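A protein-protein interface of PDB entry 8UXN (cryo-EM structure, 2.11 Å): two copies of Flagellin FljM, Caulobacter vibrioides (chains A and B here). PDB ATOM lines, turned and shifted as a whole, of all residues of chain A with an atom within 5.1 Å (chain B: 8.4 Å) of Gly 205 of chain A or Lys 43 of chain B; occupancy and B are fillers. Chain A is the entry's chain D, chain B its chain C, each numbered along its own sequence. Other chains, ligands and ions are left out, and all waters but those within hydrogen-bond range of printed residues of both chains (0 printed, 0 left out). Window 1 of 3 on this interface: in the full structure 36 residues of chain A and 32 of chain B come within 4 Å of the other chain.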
ATOM      1  N   ILE A  76     -28.796  10.827  -8.523  1.00  0.00           N
ATOM      2  CA  ILE A  76     -28.703   9.470  -8.005  1.00  0.00           C
ATOM      3  C   ILE A  76     -28.118   9.454  -6.596  1.00  0.00           C
ATOM      4  O   ILE A  76     -28.508   8.623  -5.776  1.00  0.00           O
ATOM      5  CB  ILE A  76     -27.898   8.587  -8.976  1.00  0.00           C
ATOM      6  CG1 ILE A  76     -28.666   8.398 -10.284  1.00  0.00           C
ATOM      7  CG2 ILE A  76     -27.558   7.247  -8.345  1.00  0.00           C
ATOM      8  CD1 ILE A  76     -27.868   7.783 -11.373  1.00  0.00           C
ATOM      9  N   ASP A  77     -27.202  10.372  -6.276  1.00  0.00           N
ATOM     10  CA  ASP A  77     -26.660  10.427  -4.921  1.00  0.00           C
ATOM     11  C   ASP A  77     -27.753  10.719  -3.903  1.00  0.00           C
ATOM     12  O   ASP A  77     -27.803  10.097  -2.835  1.00  0.00           O
ATOM     13  CB  ASP A  77     -25.578  11.502  -4.822  1.00  0.00           C
ATOM     14  CG  ASP A  77     -24.202  10.992  -5.170  1.00  0.00           C
ATOM     15  OD1 ASP A  77     -23.923   9.798  -4.952  1.00  0.00           O
ATOM     16  OD2 ASP A  77     -23.380  11.799  -5.650  1.00  0.00           O
ATOM     17  N   LEU A  80     -29.774   7.625  -3.399  1.00  0.00           N
ATOM     18  CA  LEU A  80     -29.105   6.618  -2.584  1.00  0.00           C
ATOM     19  C   LEU A  80     -29.106   6.981  -1.105  1.00  0.00           C
ATOM     20  O   LEU A  80     -29.205   6.091  -0.260  1.00  0.00           O
ATOM     21  CB  LEU A  80     -27.681   6.390  -3.078  1.00  0.00           C
ATOM     22  CG  LEU A  80     -27.526   5.788  -4.475  1.00  0.00           C
ATOM     23  CD1 LEU A  80     -26.084   5.847  -4.897  1.00  0.00           C
ATOM     24  CD2 LEU A  80     -28.058   4.372  -4.554  1.00  0.00           C
ATOM     25  N   LEU A 201     -31.910   0.016  -5.640  1.00  0.00           N
ATOM     26  CA  LEU A 201     -30.755   0.830  -5.293  1.00  0.00           C
ATOM     27  C   LEU A 201     -29.489   0.317  -5.966  1.00  0.00           C
ATOM     28  O   LEU A 201     -28.634   1.109  -6.369  1.00  0.00           O
ATOM     29  CB  LEU A 201     -30.598   0.880  -3.775  1.00  0.00           C
ATOM     30  CG  LEU A 201     -31.691   1.669  -3.060  1.00  0.00           C
ATOM     31  CD1 LEU A 201     -31.693   1.399  -1.574  1.00  0.00           C
ATOM     32  CD2 LEU A 201     -31.549   3.142  -3.338  1.00  0.00           C
ATOM     33  N   ALA A 202     -29.358  -1.001  -6.122  1.00  0.00           N
ATOM     34  CA  ALA A 202     -28.203  -1.534  -6.830  1.00  0.00           C
ATOM     35  C   ALA A 202     -28.225  -1.126  -8.294  1.00  0.00           C
ATOM     36  O   ALA A 202     -27.179  -0.804  -8.872  1.00  0.00           O
ATOM     37  CB  ALA A 202     -28.155  -3.050  -6.691  1.00  0.00           C
ATOM     38  N   SER A 203     -29.412  -1.089  -8.899  1.00  0.00           N
ATOM     39  CA  SER A 203     -29.505  -0.610 -10.271  1.00  0.00           C
ATOM     40  C   SER A 203     -29.148   0.864 -10.369  1.00  0.00           C
ATOM     41  O   SER A 203     -28.462   1.276 -11.306  1.00  0.00           O
ATOM     42  CB  SER A 203     -30.906  -0.847 -10.821  1.00  0.00           C
ATOM     43  OG  SER A 203     -31.098  -2.210 -11.101  1.00  0.00           O
ATOM     44  N   LEU A 204     -29.593   1.672  -9.408  1.00  0.00           N
ATOM     45  CA  LEU A 204     -29.240   3.086  -9.444  1.00  0.00           C
ATOM     46  C   LEU A 204     -27.740   3.285  -9.264  1.00  0.00           C
ATOM     47  O   LEU A 204     -27.149   4.170  -9.887  1.00  0.00           O
ATOM     48  CB  LEU A 204     -30.013   3.855  -8.378  1.00  0.00           C
ATOM     49  CG  LEU A 204     -31.492   4.135  -8.627  1.00  0.00           C
ATOM     50  CD1 LEU A 204     -32.071   4.894  -7.465  1.00  0.00           C
ATOM     51  CD2 LEU A 204     -31.721   4.886  -9.922  1.00  0.00           C
ATOM     52  N   GLY A 205     -27.098   2.451  -8.448  1.00  0.00           N
ATOM     53  CA  GLY A 205     -25.663   2.574  -8.279  1.00  0.00           C
ATOM     54  C   GLY A 205     -24.899   2.184  -9.527  1.00  0.00           C
ATOM     55  O   GLY A 205     -23.921   2.838  -9.902  1.00  0.00           O
ATOM     56  N   THR A 206     -25.358   1.138 -10.213  1.00  0.00           N
ATOM     57  CA  THR A 206     -24.740   0.787 -11.485  1.00  0.00           C
ATOM     58  C   THR A 206     -24.955   1.880 -12.527  1.00  0.00           C
ATOM     59  O   THR A 206     -24.057   2.168 -13.322  1.00  0.00           O
ATOM     60  CB  THR A 206     -25.279  -0.555 -11.971  1.00  0.00           C
ATOM     61  OG1 THR A 206     -24.925  -1.568 -11.031  1.00  0.00           O
ATOM     62  CG2 THR A 206     -24.682  -0.915 -13.294  1.00  0.00           C
ATOM     63  N   SER A 207     -26.118   2.531 -12.508  1.00  0.00           N
ATOM     64  CA  SER A 207     -26.347   3.648 -13.421  1.00  0.00           C
ATOM     65  C   SER A 207     -25.451   4.832 -13.103  1.00  0.00           C
ATOM     66  O   SER A 207     -24.996   5.528 -14.013  1.00  0.00           O
ATOM     67  CB  SER A 207     -27.806   4.086 -13.368  1.00  0.00           C
ATOM     68  OG  SER A 207     -28.652   3.067 -13.825  1.00  0.00           O
ATOM     69  N   SER A 208     -25.186   5.075 -11.826  1.00  0.00           N
ATOM     70  CA  SER A 208     -24.294   6.164 -11.463  1.00  0.00           C
ATOM     71  C   SER A 208     -22.876   5.879 -11.933  1.00  0.00           C
ATOM     72  O   SER A 208     -22.199   6.765 -12.469  1.00  0.00           O
ATOM     73  CB  SER A 208     -24.339   6.386  -9.955  1.00  0.00           C
ATOM     74  OG  SER A 208     -23.609   7.529  -9.585  1.00  0.00           O
ATOM     75  N   THR A 209     -22.423   4.636 -11.765  1.00  0.00           N
ATOM     76  CA  THR A 209     -21.099   4.269 -12.250  1.00  0.00           C
ATOM     77  C   THR A 209     -21.018   4.347 -13.770  1.00  0.00           C
ATOM     78  O   THR A 209     -19.990   4.763 -14.313  1.00  0.00           O
ATOM     79  CB  THR A 209     -20.731   2.872 -11.756  1.00  0.00           C
ATOM     80  OG1 THR A 209     -20.695   2.874 -10.328  1.00  0.00           O
ATOM     81  CG2 THR A 209     -19.380   2.462 -12.261  1.00  0.00           C
ATOM     82  N   GLY A 210     -22.103   4.015 -14.467  1.00  0.00           N
ATOM     83  CA  GLY A 210     -22.105   4.151 -15.911  1.00  0.00           C
ATOM     84  C   GLY A 210     -22.053   5.598 -16.355  1.00  0.00           C
ATOM     85  O   GLY A 210     -21.368   5.933 -17.322  1.00  0.00           O
ATOM     86  N   GLN B  31     -12.093   6.642   0.582  1.00  0.00           N
ATOM     87  CA  GLN B  31     -13.396   6.149   1.012  1.00  0.00           C
ATOM     88  C   GLN B  31     -13.270   4.805   1.714  1.00  0.00           C
ATOM     89  O   GLN B  31     -13.908   4.578   2.749  1.00  0.00           O
ATOM     90  CB  GLN B  31     -14.344   6.051  -0.175  1.00  0.00           C
ATOM     91  CG  GLN B  31     -14.723   7.389  -0.758  1.00  0.00           C
ATOM     92  CD  GLN B  31     -15.435   7.267  -2.082  1.00  0.00           C
ATOM     93  OE1 GLN B  31     -15.542   6.179  -2.647  1.00  0.00           O
ATOM     94  NE2 GLN B  31     -15.912   8.389  -2.600  1.00  0.00           N
ATOM     95  N   LYS B  38     -14.628  -2.027   1.411  1.00  0.00           N
ATOM     96  CA  LYS B  38     -14.368  -2.005  -0.019  1.00  0.00           C
ATOM     97  C   LYS B  38     -15.645  -1.883  -0.838  1.00  0.00           C
ATOM     98  O   LYS B  38     -15.592  -1.400  -1.968  1.00  0.00           O
ATOM     99  CB  LYS B  38     -13.571  -3.237  -0.445  1.00  0.00           C
ATOM    100  CG  LYS B  38     -14.219  -4.570  -0.185  1.00  0.00           C
ATOM    101  CD  LYS B  38     -13.303  -5.675  -0.641  1.00  0.00           C
ATOM    102  CE  LYS B  38     -13.970  -7.038  -0.611  1.00  0.00           C
ATOM    103  NZ  LYS B  38     -14.195  -7.516   0.764  1.00  0.00           N
ATOM    104  N   ILE B  39     -16.788  -2.275  -0.290  1.00  0.00           N
ATOM    105  CA  ILE B  39     -18.085  -2.085  -0.936  1.00  0.00           C
ATOM    106  C   ILE B  39     -18.950  -1.344   0.076  1.00  0.00           C
ATOM    107  O   ILE B  39     -19.621  -1.952   0.912  1.00  0.00           O
ATOM    108  CB  ILE B  39     -18.728  -3.403  -1.385  1.00  0.00           C
ATOM    109  CG1 ILE B  39     -17.911  -4.023  -2.516  1.00  0.00           C
ATOM    110  CG2 ILE B  39     -20.148  -3.189  -1.872  1.00  0.00           C
ATOM    111  CD1 ILE B  39     -17.839  -5.496  -2.478  1.00  0.00           C
ATOM    112  N   GLY B  40     -18.896  -0.020   0.040  1.00  0.00           N
ATOM    113  CA  GLY B  40     -19.630   0.802   0.975  1.00  0.00           C
ATOM    114  C   GLY B  40     -20.944   1.332   0.487  1.00  0.00           C
ATOM    115  O   GLY B  40     -21.705   1.882   1.274  1.00  0.00           O
ATOM    116  N   SER B  41     -21.246   1.172  -0.793  1.00  0.00           N
ATOM    117  CA  SER B  41     -22.479   1.694  -1.354  1.00  0.00           C
ATOM    118  C   SER B  41     -22.836   0.871  -2.577  1.00  0.00           C
ATOM    119  O   SER B  41     -22.064   0.027  -3.030  1.00  0.00           O
ATOM    120  CB  SER B  41     -22.359   3.180  -1.701  1.00  0.00           C
ATOM    121  OG  SER B  41     -21.704   3.371  -2.932  1.00  0.00           O
ATOM    122  N   ALA B  42     -24.033   1.118  -3.096  1.00  0.00           N
ATOM    123  CA  ALA B  42     -24.473   0.433  -4.301  1.00  0.00           C
ATOM    124  C   ALA B  42     -23.592   0.768  -5.498  1.00  0.00           C
ATOM    125  O   ALA B  42     -23.487  -0.032  -6.428  1.00  0.00           O
ATOM    126  CB  ALA B  42     -25.928   0.788  -4.589  1.00  0.00           C
ATOM    127  N   LYS B  43     -22.954   1.936  -5.497  1.00  0.00           N
ATOM    128  CA  LYS B  43     -22.078   2.307  -6.603  1.00  0.00           C
ATOM    129  C   LYS B  43     -20.832   1.432  -6.688  1.00  0.00           C
ATOM    130  O   LYS B  43     -20.269   1.282  -7.772  1.00  0.00           O
ATOM    131  CB  LYS B  43     -21.672   3.771  -6.482  1.00  0.00           C
ATOM    132  CG  LYS B  43     -22.796   4.735  -6.715  1.00  0.00           C
ATOM    133  CD  LYS B  43     -22.314   6.161  -6.628  1.00  0.00           C
ATOM    134  CE  LYS B  43     -22.012   6.546  -5.202  1.00  0.00           C
ATOM    135  NZ  LYS B  43     -21.564   7.951  -5.100  1.00  0.00           N
ATOM    136  N   ASP B  44     -20.381   0.855  -5.576  1.00  0.00           N
ATOM    137  CA  ASP B  44     -19.126   0.108  -5.590  1.00  0.00           C
ATOM    138  C   ASP B  44     -19.266  -1.229  -6.305  1.00  0.00           C
ATOM    139  O   ASP B  44     -18.381  -1.624  -7.067  1.00  0.00           O
ATOM    140  CB  ASP B  44     -18.630  -0.106  -4.162  1.00  0.00           C
ATOM    141  CG  ASP B  44     -18.146   1.167  -3.523  1.00  0.00           C
ATOM    142  OD1 ASP B  44     -17.697   2.064  -4.259  1.00  0.00           O
ATOM    143  OD2 ASP B  44     -18.218   1.284  -2.288  1.00  0.00           O
ATOM    144  N   ASN B  45     -20.368  -1.932  -6.072  1.00  0.00           N
ATOM    145  CA  ASN B  45     -20.654  -3.242  -6.645  1.00  0.00           C
ATOM    146  C   ASN B  45     -22.079  -3.575  -6.247  1.00  0.00           C
ATOM    147  O   ASN B  45     -22.310  -4.056  -5.139  1.00  0.00           O
ATOM    148  CB  ASN B  45     -19.672  -4.302  -6.137  1.00  0.00           C
ATOM    149  CG  ASN B  45     -19.901  -5.679  -6.742  1.00  0.00           C
ATOM    150  OD1 ASN B  45     -21.023  -6.082  -7.014  1.00  0.00           O
ATOM    151  ND2 ASN B  45     -18.828  -6.414  -6.927  1.00  0.00           N
ATOM    152  N   GLY B  46     -23.034  -3.319  -7.134  1.00  0.00           N
ATOM    153  CA  GLY B  46     -24.423  -3.298  -6.716  1.00  0.00           C
ATOM    154  C   GLY B  46     -24.931  -4.645  -6.246  1.00  0.00           C
ATOM    155  O   GLY B  46     -25.655  -4.724  -5.255  1.00  0.00           O
ATOM    156  N   ALA B  47     -24.519  -5.723  -6.911  1.00  0.00           N
ATOM    157  CA  ALA B  47     -25.017  -7.043  -6.549  1.00  0.00           C
ATOM    158  C   ALA B  47     -24.506  -7.476  -5.181  1.00  0.00           C
ATOM    159  O   ALA B  47     -25.285  -7.918  -4.329  1.00  0.00           O
ATOM    160  CB  ALA B  47     -24.627  -8.063  -7.614  1.00  0.00           C
ATOM    161  N   TRP B  49     -23.324  -5.540  -2.878  1.00  0.00           N
ATOM    162  CA  TRP B  49     -23.852  -4.609  -1.890  1.00  0.00           C
ATOM    163  C   TRP B  49     -25.264  -4.996  -1.474  1.00  0.00           C
ATOM    164  O   TRP B  49     -25.584  -5.008  -0.284  1.00  0.00           O
ATOM    165  CB  TRP B  49     -23.825  -3.183  -2.436  1.00  0.00           C
ATOM    166  CG  TRP B  49     -24.506  -2.198  -1.558  1.00  0.00           C
ATOM    167  CD1 TRP B  49     -23.956  -1.511  -0.529  1.00  0.00           C
ATOM    168  CD2 TRP B  49     -25.870  -1.791  -1.627  1.00  0.00           C
ATOM    169  NE1 TRP B  49     -24.884  -0.698   0.046  1.00  0.00           N
ATOM    170  CE2 TRP B  49     -26.072  -0.851  -0.609  1.00  0.00           C
ATOM    171  CE3 TRP B  49     -26.942  -2.131  -2.453  1.00  0.00           C
ATOM    172  CZ2 TRP B  49     -27.299  -0.246  -0.392  1.00  0.00           C
ATOM    173  CZ3 TRP B  49     -28.155  -1.536  -2.234  1.00  0.00           C
ATOM    174  CH2 TRP B  49     -28.326  -0.600  -1.213  1.00  0.00           C
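NZ of Lys 43 of chain B is in salt-bridge range of OD1 of Asp 77 of chain A, at 3.0 Å. The backbone carbonyl oxygen (O) of Lys 43 of chain B is in hydrogen-bond range of the side-chain hydroxyl (OG1) of Thr 209 of chain A (3.0 Å).
The backbone NH (N) of Lys 43 of chain B lies close to the side-chain hydroxyl (OG) of Ser 41 of chain B. O of Ala 202 of chain A lies within hydrogen-bond range of OG1 of Thr 206 of chain A (3.2 Å). O of Gly 205 of chain A is in hydrogen-bond range of OG1 of Thr 209 of chain A (3.3 Å).
Lys 43 of chain B touches Leu 80 of chain A. Ala 42 of chain B touches Leu 201 of chain A (CB to O, 3.3 Å). CH2 of Trp 49 of chain B touches CB of Leu 201 of chain A, at 3.7 Å. Ala 202 of chain A touches Ala 42 of chain B (CA to CB, 3.9 Å). Ala 202 of chain A touches Gly 46 of chain B. Gly 205 of chain A touches Ala 42 of chain B (CA to O, 3.9 Å). Lys 43 of chain B touches Gly 205 of chain A. Ser 208 of chain A touches Lys 43 of chain B (OG to CD, 3.5 Å).
Of chain B, only Ala 42 (3.9 Å) and Lys 43 (3.8 Å) come within 4 Å of Gly 205 of chain A. Lys 43 of chain B touches just these residues of chain A: Asp 77, Leu 80, Gly 205, Ser 208 and Thr 209. Of the printed residues of chain B, Ala 202 of chain A touches Ala 42 (3.9 Å) and Gly 46 (3.3 Å). Of the printed residues of chain B, Leu 80 of chain A touches Lys 43. Of the printed residues of chain B, Leu 201 of chain A touches Ala 42 and Trp 49. Of the printed residues of chain B, Thr 209 of chain A touches Lys 43. Printed residues of chain B within 4 Å of Asp 77 of chain A: Lys 43 (3.0 Å). The nearest residue of chain B that does not touch Gly 205 of chain A is Asp 44 of chain B (5.9 Å). The nearest residue of chain A that does not touch Lys 43 of chain B is Thr 206 of chain A (5.0 Å).
Of the 13 printed residues of chain A, 7 touch a printed residue of chain B. Among the printed residues, 10 pairs touch across the chains. Among the printed residues, Asp or Glu carboxylates within 4 Å of a Lys or Arg side-chain nitrogen of the other chain: Asp 77 of chain A with Lys 43 of chain B (3.0 Å).
No position is printed for both chains.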
